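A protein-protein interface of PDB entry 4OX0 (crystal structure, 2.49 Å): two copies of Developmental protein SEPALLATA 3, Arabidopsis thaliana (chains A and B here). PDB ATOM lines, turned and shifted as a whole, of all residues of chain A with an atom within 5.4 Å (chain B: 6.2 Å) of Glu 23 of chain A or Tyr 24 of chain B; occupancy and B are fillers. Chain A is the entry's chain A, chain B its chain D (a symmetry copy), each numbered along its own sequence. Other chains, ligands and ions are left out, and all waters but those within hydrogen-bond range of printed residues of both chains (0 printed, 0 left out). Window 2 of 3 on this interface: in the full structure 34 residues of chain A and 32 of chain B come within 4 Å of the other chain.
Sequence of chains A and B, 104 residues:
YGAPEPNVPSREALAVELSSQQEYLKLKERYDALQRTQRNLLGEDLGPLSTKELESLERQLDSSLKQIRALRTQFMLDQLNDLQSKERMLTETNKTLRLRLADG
The side-chain hydroxyl of Ser 20 of chain A sits at hydrogen-bond distance from the side-chain hydroxyl of Ser 20 of chain B.
Glu 23 of chain A touches Tyr 24 of chain B, and with the chains exchanged Tyr 24 of chain A touches Glu 23 of chain B.
Tyr 24 of chain B touches its own counterpart, Tyr 24 of chain A.
Tyr 24 of chain A touches Leu 27 of chain B, and with the chains exchanged Leu 27 of chain A touches Tyr 24 of chain B.
Leu 27 of chain A touches Lys 28 of chain B, and with the chains exchanged Lys 28 of chain A touches Leu 27 of chain B.
Among the printed residues, 9 pairs touch across the chains.
Among the printed residues, merely in contact across the chains: Glu 23 of chain A with Tyr 24 of chain B (3.3 Å), Tyr 24 of chain A with Glu 23 of chain B (3.1 Å), Tyr 24 of chain A with Tyr 24 of chain B (3.9 Å), Tyr 24 of chain A with Leu 27 of chain B (3.7 Å), Leu 27 of chain A with Tyr 24 of chain B (3.7 Å), Leu 27 of chain A with Leu 27 of chain B (3.7 Å), Leu 27 of chain A with Lys 28 of chain B (3.8 Å) and Lys 28 of chain A with Leu 27 of chain B (3.7 Å).
Of chain B, only Tyr 24 (3.3 Å) comes within 4 Å of Glu 23 of chain A.
Of the printed residues of chain B, Leu 27 of chain A touches Tyr 24, Leu 27 and Lys 28.
Of the printed residues of chain B, Lys 28 of chain A touches Leu 27.
Tyr 24 of chain B touches three residues of chain A.
The nearest printed residue of chain B that does not touch Glu 23 of chain A is Leu 27 of chain B (6.5 Å).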
ATOM      1  N   SER A  19     -33.396 -20.475   8.634  1.00  0.00           N
ATOM      2  CA  SER A  19     -32.188 -20.265   9.447  1.00  0.00           C
ATOM      3  C   SER A  19     -30.994 -20.030   8.530  1.00  0.00           C
ATOM      4  O   SER A  19     -30.112 -19.238   8.871  1.00  0.00           O
ATOM      5  CB  SER A  19     -31.919 -21.468  10.347  1.00  0.00           C
ATOM      6  OG  SER A  19     -31.270 -21.097  11.551  1.00  0.00           O
ATOM      7  N   SER A  20     -30.977 -20.713   7.359  1.00  0.00           N
ATOM      8  CA  SER A  20     -29.944 -20.580   6.324  1.00  0.00           C
ATOM      9  C   SER A  20     -30.082 -19.219   5.615  1.00  0.00           C
ATOM     10  O   SER A  20     -29.080 -18.601   5.267  1.00  0.00           O
ATOM     11  CB  SER A  20     -30.028 -21.735   5.327  1.00  0.00           C
ATOM     12  OG  SER A  20     -30.898 -21.470   4.237  1.00  0.00           O
ATOM     13  N   GLN A  21     -31.337 -18.763   5.421  1.00  0.00           N
ATOM     14  CA  GLN A  21     -31.697 -17.473   4.829  1.00  0.00           C
ATOM     15  C   GLN A  21     -31.211 -16.347   5.741  1.00  0.00           C
ATOM     16  O   GLN A  21     -30.899 -15.263   5.257  1.00  0.00           O
ATOM     17  CB  GLN A  21     -33.227 -17.358   4.661  1.00  0.00           C
ATOM     18  CG  GLN A  21     -33.799 -18.064   3.430  1.00  0.00           C
ATOM     19  CD  GLN A  21     -35.273 -17.774   3.191  1.00  0.00           C
ATOM     20  OE1 GLN A  21     -35.807 -16.713   3.553  1.00  0.00           O
ATOM     21  NE2 GLN A  21     -35.961 -18.699   2.530  1.00  0.00           N
ATOM     22  N   GLN A  22     -31.168 -16.612   7.064  1.00  0.00           N
ATOM     23  CA  GLN A  22     -30.735 -15.681   8.103  1.00  0.00           C
ATOM     24  C   GLN A  22     -29.230 -15.468   8.044  1.00  0.00           C
ATOM     25  O   GLN A  22     -28.779 -14.318   8.054  1.00  0.00           O
ATOM     26  CB  GLN A  22     -31.179 -16.173   9.498  1.00  0.00           C
ATOM     27  CG  GLN A  22     -32.311 -15.348  10.113  1.00  0.00           C
ATOM     28  CD  GLN A  22     -31.894 -13.913  10.383  1.00  0.00           C
ATOM     29  OE1 GLN A  22     -30.949 -13.640  11.134  1.00  0.00           O
ATOM     30  NE2 GLN A  22     -32.580 -12.966   9.755  1.00  0.00           N
ATOM     31  N   GLU A  23     -28.449 -16.571   7.947  1.00  0.00           N
ATOM     32  CA  GLU A  23     -26.992 -16.506   7.851  1.00  0.00           C
ATOM     33  C   GLU A  23     -26.524 -16.034   6.470  1.00  0.00           C
ATOM     34  O   GLU A  23     -25.412 -15.494   6.343  1.00  0.00           O
ATOM     35  CB  GLU A  23     -26.307 -17.797   8.338  1.00  0.00           C
ATOM     36  CG  GLU A  23     -26.420 -19.008   7.425  1.00  0.00           C
ATOM     37  CD  GLU A  23     -25.608 -20.223   7.843  1.00  0.00           C
ATOM     38  OE1 GLU A  23     -24.697 -20.083   8.693  1.00  0.00           O
ATOM     39  OE2 GLU A  23     -25.860 -21.316   7.287  1.00  0.00           O
ATOM     40  N   TYR A  24     -27.386 -16.195   5.444  1.00  0.00           N
ATOM     41  CA  TYR A  24     -27.091 -15.708   4.099  1.00  0.00           C
ATOM     42  C   TYR A  24     -27.244 -14.194   4.089  1.00  0.00           C
ATOM     43  O   TYR A  24     -26.400 -13.512   3.529  1.00  0.00           O
ATOM     44  CB  TYR A  24     -27.987 -16.365   3.044  1.00  0.00           C
ATOM     45  CG  TYR A  24     -27.548 -16.094   1.625  1.00  0.00           C
ATOM     46  CD1 TYR A  24     -26.584 -16.891   1.007  1.00  0.00           C
ATOM     47  CD2 TYR A  24     -28.111 -15.062   0.884  1.00  0.00           C
ATOM     48  CE1 TYR A  24     -26.173 -16.647  -0.305  1.00  0.00           C
ATOM     49  CE2 TYR A  24     -27.694 -14.795  -0.422  1.00  0.00           C
ATOM     50  CZ  TYR A  24     -26.731 -15.598  -1.018  1.00  0.00           C
ATOM     51  OH  TYR A  24     -26.324 -15.346  -2.310  1.00  0.00           O
ATOM     52  N   LEU A  25     -28.271 -13.663   4.761  1.00  0.00           N
ATOM     53  CA  LEU A  25     -28.489 -12.221   4.861  1.00  0.00           C
ATOM     54  C   LEU A  25     -27.473 -11.531   5.770  1.00  0.00           C
ATOM     55  O   LEU A  25     -27.329 -10.308   5.711  1.00  0.00           O
ATOM     56  CB  LEU A  25     -29.928 -11.911   5.269  1.00  0.00           C
ATOM     57  CG  LEU A  25     -30.719 -11.041   4.294  1.00  0.00           C
ATOM     58  CD1 LEU A  25     -30.610 -11.548   2.846  1.00  0.00           C
ATOM     59  CD2 LEU A  25     -32.180 -10.951   4.716  1.00  0.00           C
ATOM     60  N   LYS A  26     -26.740 -12.321   6.580  1.00  0.00           N
ATOM     61  CA  LYS A  26     -25.660 -11.842   7.441  1.00  0.00           C
ATOM     62  C   LYS A  26     -24.379 -11.737   6.586  1.00  0.00           C
ATOM     63  O   LYS A  26     -23.638 -10.759   6.712  1.00  0.00           O
ATOM     64  CB  LYS A  26     -25.453 -12.772   8.654  1.00  0.00           C
ATOM     65  CG  LYS A  26     -26.475 -12.546   9.775  1.00  0.00           C
ATOM     66  CD  LYS A  26     -25.848 -12.561  11.181  1.00  0.00           C
ATOM     67  CE  LYS A  26     -25.220 -11.239  11.587  1.00  0.00           C
ATOM     68  NZ  LYS A  26     -24.690 -11.270  12.977  1.00  0.00           N
ATOM     69  N   LEU A  27     -24.163 -12.736   5.692  1.00  0.00           N
ATOM     70  CA  LEU A  27     -23.043 -12.822   4.762  1.00  0.00           C
ATOM     71  C   LEU A  27     -23.204 -11.826   3.610  1.00  0.00           C
ATOM     72  O   LEU A  27     -22.215 -11.190   3.239  1.00  0.00           O
ATOM     73  CB  LEU A  27     -22.853 -14.259   4.241  1.00  0.00           C
ATOM     74  CG  LEU A  27     -21.610 -14.552   3.367  1.00  0.00           C
ATOM     75  CD1 LEU A  27     -20.285 -14.406   4.152  1.00  0.00           C
ATOM     76  CD2 LEU A  27     -21.697 -15.929   2.746  1.00  0.00           C
ATOM     77  N   LYS A  28     -24.428 -11.672   3.052  1.00  0.00           N
ATOM     78  CA  LYS A  28     -24.705 -10.723   1.959  1.00  0.00           C
ATOM     79  C   LYS A  28     -24.395  -9.301   2.407  1.00  0.00           C
ATOM     80  O   LYS A  28     -23.787  -8.552   1.646  1.00  0.00           O
ATOM     81  CB  LYS A  28     -26.160 -10.843   1.445  1.00  0.00           C
ATOM     82  CG  LYS A  28     -26.531  -9.903   0.285  1.00  0.00           C
ATOM     83  CD  LYS A  28     -26.210 -10.440  -1.113  1.00  0.00           C
ATOM     84  CE  LYS A  28     -25.232  -9.570  -1.860  1.00  0.00           C
ATOM     85  NZ  LYS A  28     -24.785 -10.190  -3.133  1.00  0.00           N
ATOM     86  N   SER B  20     -30.467 -23.850  -1.514  1.00  0.00           N
ATOM     87  CA  SER B  20     -30.231 -22.748  -0.570  1.00  0.00           C
ATOM     88  C   SER B  20     -28.907 -22.916   0.200  1.00  0.00           C
ATOM     89  O   SER B  20     -28.215 -21.920   0.448  1.00  0.00           O
ATOM     90  CB  SER B  20     -31.405 -22.600   0.396  1.00  0.00           C
ATOM     91  OG  SER B  20     -31.478 -21.298   0.955  1.00  0.00           O
ATOM     92  N   GLN B  21     -28.560 -24.179   0.564  1.00  0.00           N
ATOM     93  CA  GLN B  21     -27.331 -24.532   1.289  1.00  0.00           C
ATOM     94  C   GLN B  21     -26.050 -24.199   0.487  1.00  0.00           C
ATOM     95  O   GLN B  21     -25.150 -23.544   1.021  1.00  0.00           O
ATOM     96  CB  GLN B  21     -27.352 -26.012   1.729  1.00  0.00           C
ATOM     97  CG  GLN B  21     -28.321 -26.300   2.884  1.00  0.00           C
ATOM     98  CD  GLN B  21     -28.581 -27.777   3.154  1.00  0.00           C
ATOM     99  OE1 GLN B  21     -29.726 -28.200   3.351  1.00  0.00           O
ATOM    100  NE2 GLN B  21     -27.532 -28.591   3.225  1.00  0.00           N
ATOM    101  N   GLN B  22     -25.996 -24.628  -0.797  1.00  0.00           N
ATOM    102  CA  GLN B  22     -24.866 -24.413  -1.717  1.00  0.00           C
ATOM    103  C   GLN B  22     -24.745 -22.951  -2.153  1.00  0.00           C
ATOM    104  O   GLN B  22     -23.644 -22.501  -2.511  1.00  0.00           O
ATOM    105  CB  GLN B  22     -24.972 -25.332  -2.948  1.00  0.00           C
ATOM    106  CG  GLN B  22     -25.122 -26.816  -2.607  1.00  0.00           C
ATOM    107  CD  GLN B  22     -26.363 -27.443  -3.202  1.00  0.00           C
ATOM    108  OE1 GLN B  22     -26.310 -28.525  -3.796  1.00  0.00           O
ATOM    109  NE2 GLN B  22     -27.513 -26.798  -3.045  1.00  0.00           N
ATOM    110  N   GLU B  23     -25.878 -22.210  -2.118  1.00  0.00           N
ATOM    111  CA  GLU B  23     -25.955 -20.788  -2.484  1.00  0.00           C
ATOM    112  C   GLU B  23     -25.103 -19.897  -1.547  1.00  0.00           C
ATOM    113  O   GLU B  23     -24.692 -18.804  -1.943  1.00  0.00           O
ATOM    114  CB  GLU B  23     -27.422 -20.321  -2.519  1.00  0.00           C
ATOM    115  CG  GLU B  23     -27.687 -19.275  -3.589  1.00  0.00           C
ATOM    116  CD  GLU B  23     -29.096 -18.721  -3.633  1.00  0.00           C
ATOM    117  OE1 GLU B  23     -29.550 -18.151  -2.613  1.00  0.00           O
ATOM    118  OE2 GLU B  23     -29.730 -18.812  -4.709  1.00  0.00           O
ATOM    119  N   TYR B  24     -24.844 -20.386  -0.315  1.00  0.00           N
ATOM    120  CA  TYR B  24     -24.023 -19.756   0.719  1.00  0.00           C
ATOM    121  C   TYR B  24     -22.546 -19.952   0.362  1.00  0.00           C
ATOM    122  O   TYR B  24     -21.760 -19.003   0.489  1.00  0.00           O
ATOM    123  CB  TYR B  24     -24.313 -20.400   2.090  1.00  0.00           C
ATOM    124  CG  TYR B  24     -23.676 -19.687   3.263  1.00  0.00           C
ATOM    125  CD1 TYR B  24     -24.338 -18.652   3.917  1.00  0.00           C
ATOM    126  CD2 TYR B  24     -22.411 -20.051   3.726  1.00  0.00           C
ATOM    127  CE1 TYR B  24     -23.757 -17.995   5.002  1.00  0.00           C
ATOM    128  CE2 TYR B  24     -21.808 -19.378   4.788  1.00  0.00           C
ATOM    129  CZ  TYR B  24     -22.491 -18.361   5.432  1.00  0.00           C
ATOM    130  OH  TYR B  24     -21.917 -17.730   6.505  1.00  0.00           O
ATOM    131  N   LEU B  25     -22.169 -21.196  -0.038  1.00  0.00           N
ATOM    132  CA  LEU B  25     -20.798 -21.518  -0.425  1.00  0.00           C
ATOM    133  C   LEU B  25     -20.337 -20.680  -1.611  1.00  0.00           C
ATOM    134  O   LEU B  25     -19.247 -20.115  -1.549  1.00  0.00           O
ATOM    135  CB  LEU B  25     -20.613 -23.011  -0.670  1.00  0.00           C
ATOM    136  CG  LEU B  25     -20.253 -23.799   0.583  1.00  0.00           C
ATOM    137  CD1 LEU B  25     -20.950 -25.175   0.604  1.00  0.00           C
ATOM    138  CD2 LEU B  25     -18.722 -23.876   0.776  1.00  0.00           C
ATOM    139  N   LYS B  26     -21.220 -20.508  -2.626  1.00  0.00           N
ATOM    140  CA  LYS B  26     -21.012 -19.674  -3.813  1.00  0.00           C
ATOM    141  C   LYS B  26     -20.724 -18.219  -3.384  1.00  0.00           C
ATOM    142  O   LYS B  26     -19.767 -17.607  -3.887  1.00  0.00           O
ATOM    143  CB  LYS B  26     -22.236 -19.772  -4.761  1.00  0.00           C
ATOM    144  CG  LYS B  26     -22.290 -18.775  -5.929  1.00  0.00           C
ATOM    145  CD  LYS B  26     -21.155 -18.931  -6.959  1.00  0.00           C
ATOM    146  CE  LYS B  26     -21.032 -17.705  -7.843  1.00  0.00           C
ATOM    147  NZ  LYS B  26     -19.619 -17.276  -8.023  1.00  0.00           N
ATOM    148  N   LEU B  27     -21.512 -17.698  -2.417  1.00  0.00           N
ATOM    149  CA  LEU B  27     -21.321 -16.344  -1.902  1.00  0.00           C
ATOM    150  C   LEU B  27     -20.046 -16.240  -1.073  1.00  0.00           C
ATOM    151  O   LEU B  27     -19.319 -15.261  -1.237  1.00  0.00           O
ATOM    152  CB  LEU B  27     -22.546 -15.838  -1.112  1.00  0.00           C
ATOM    153  CG  LEU B  27     -22.548 -14.338  -0.718  1.00  0.00           C
ATOM    154  CD1 LEU B  27     -22.685 -13.429  -1.940  1.00  0.00           C
ATOM    155  CD2 LEU B  27     -23.663 -14.030   0.262  1.00  0.00           C
ATOM    156  N   LYS B  28     -19.759 -17.245  -0.203  1.00  0.00           N
ATOM    157  CA  LYS B  28     -18.544 -17.271   0.629  1.00  0.00           C
ATOM    158  C   LYS B  28     -17.289 -17.256  -0.251  1.00  0.00           C
ATOM    159  O   LYS B  28     -16.345 -16.522   0.052  1.00  0.00           O
ATOM    160  CB  LYS B  28     -18.533 -18.453   1.611  1.00  0.00           C
ATOM    161  CG  LYS B  28     -17.411 -18.337   2.638  1.00  0.00           C
ATOM    162  CD  LYS B  28     -16.877 -19.680   2.957  1.00  0.00           C
ATOM    163  CE  LYS B  28     -16.045 -19.681   4.215  1.00  0.00           C
ATOM    164  NZ  LYS B  28     -16.033 -21.027   4.866  1.00  0.00           N
ATOM    165  N   GLU B  29     -17.309 -18.023  -1.361  1.00  0.00           N
ATOM    166  CA  GLU B  29     -16.218 -18.101  -2.344  1.00  0.00           C
ATOM    167  C   GLU B  29     -15.978 -16.731  -3.005  1.00  0.00           C
ATOM    168  O   GLU B  29     -14.829 -16.352  -3.207  1.00  0.00           O
ATOM    169  CB  GLU B  29     -16.515 -19.170  -3.422  1.00  0.00           C
ATOM    170  CG  GLU B  29     -16.391 -20.615  -2.963  1.00  0.00           C
ATOM    171  CD  GLU B  29     -17.361 -21.614  -3.584  1.00  0.00           C
ATOM    172  OE1 GLU B  29     -17.757 -21.415  -4.757  1.00  0.00           O
ATOM    173  OE2 GLU B  29     -17.728 -22.596  -2.896  1.00  0.00           O
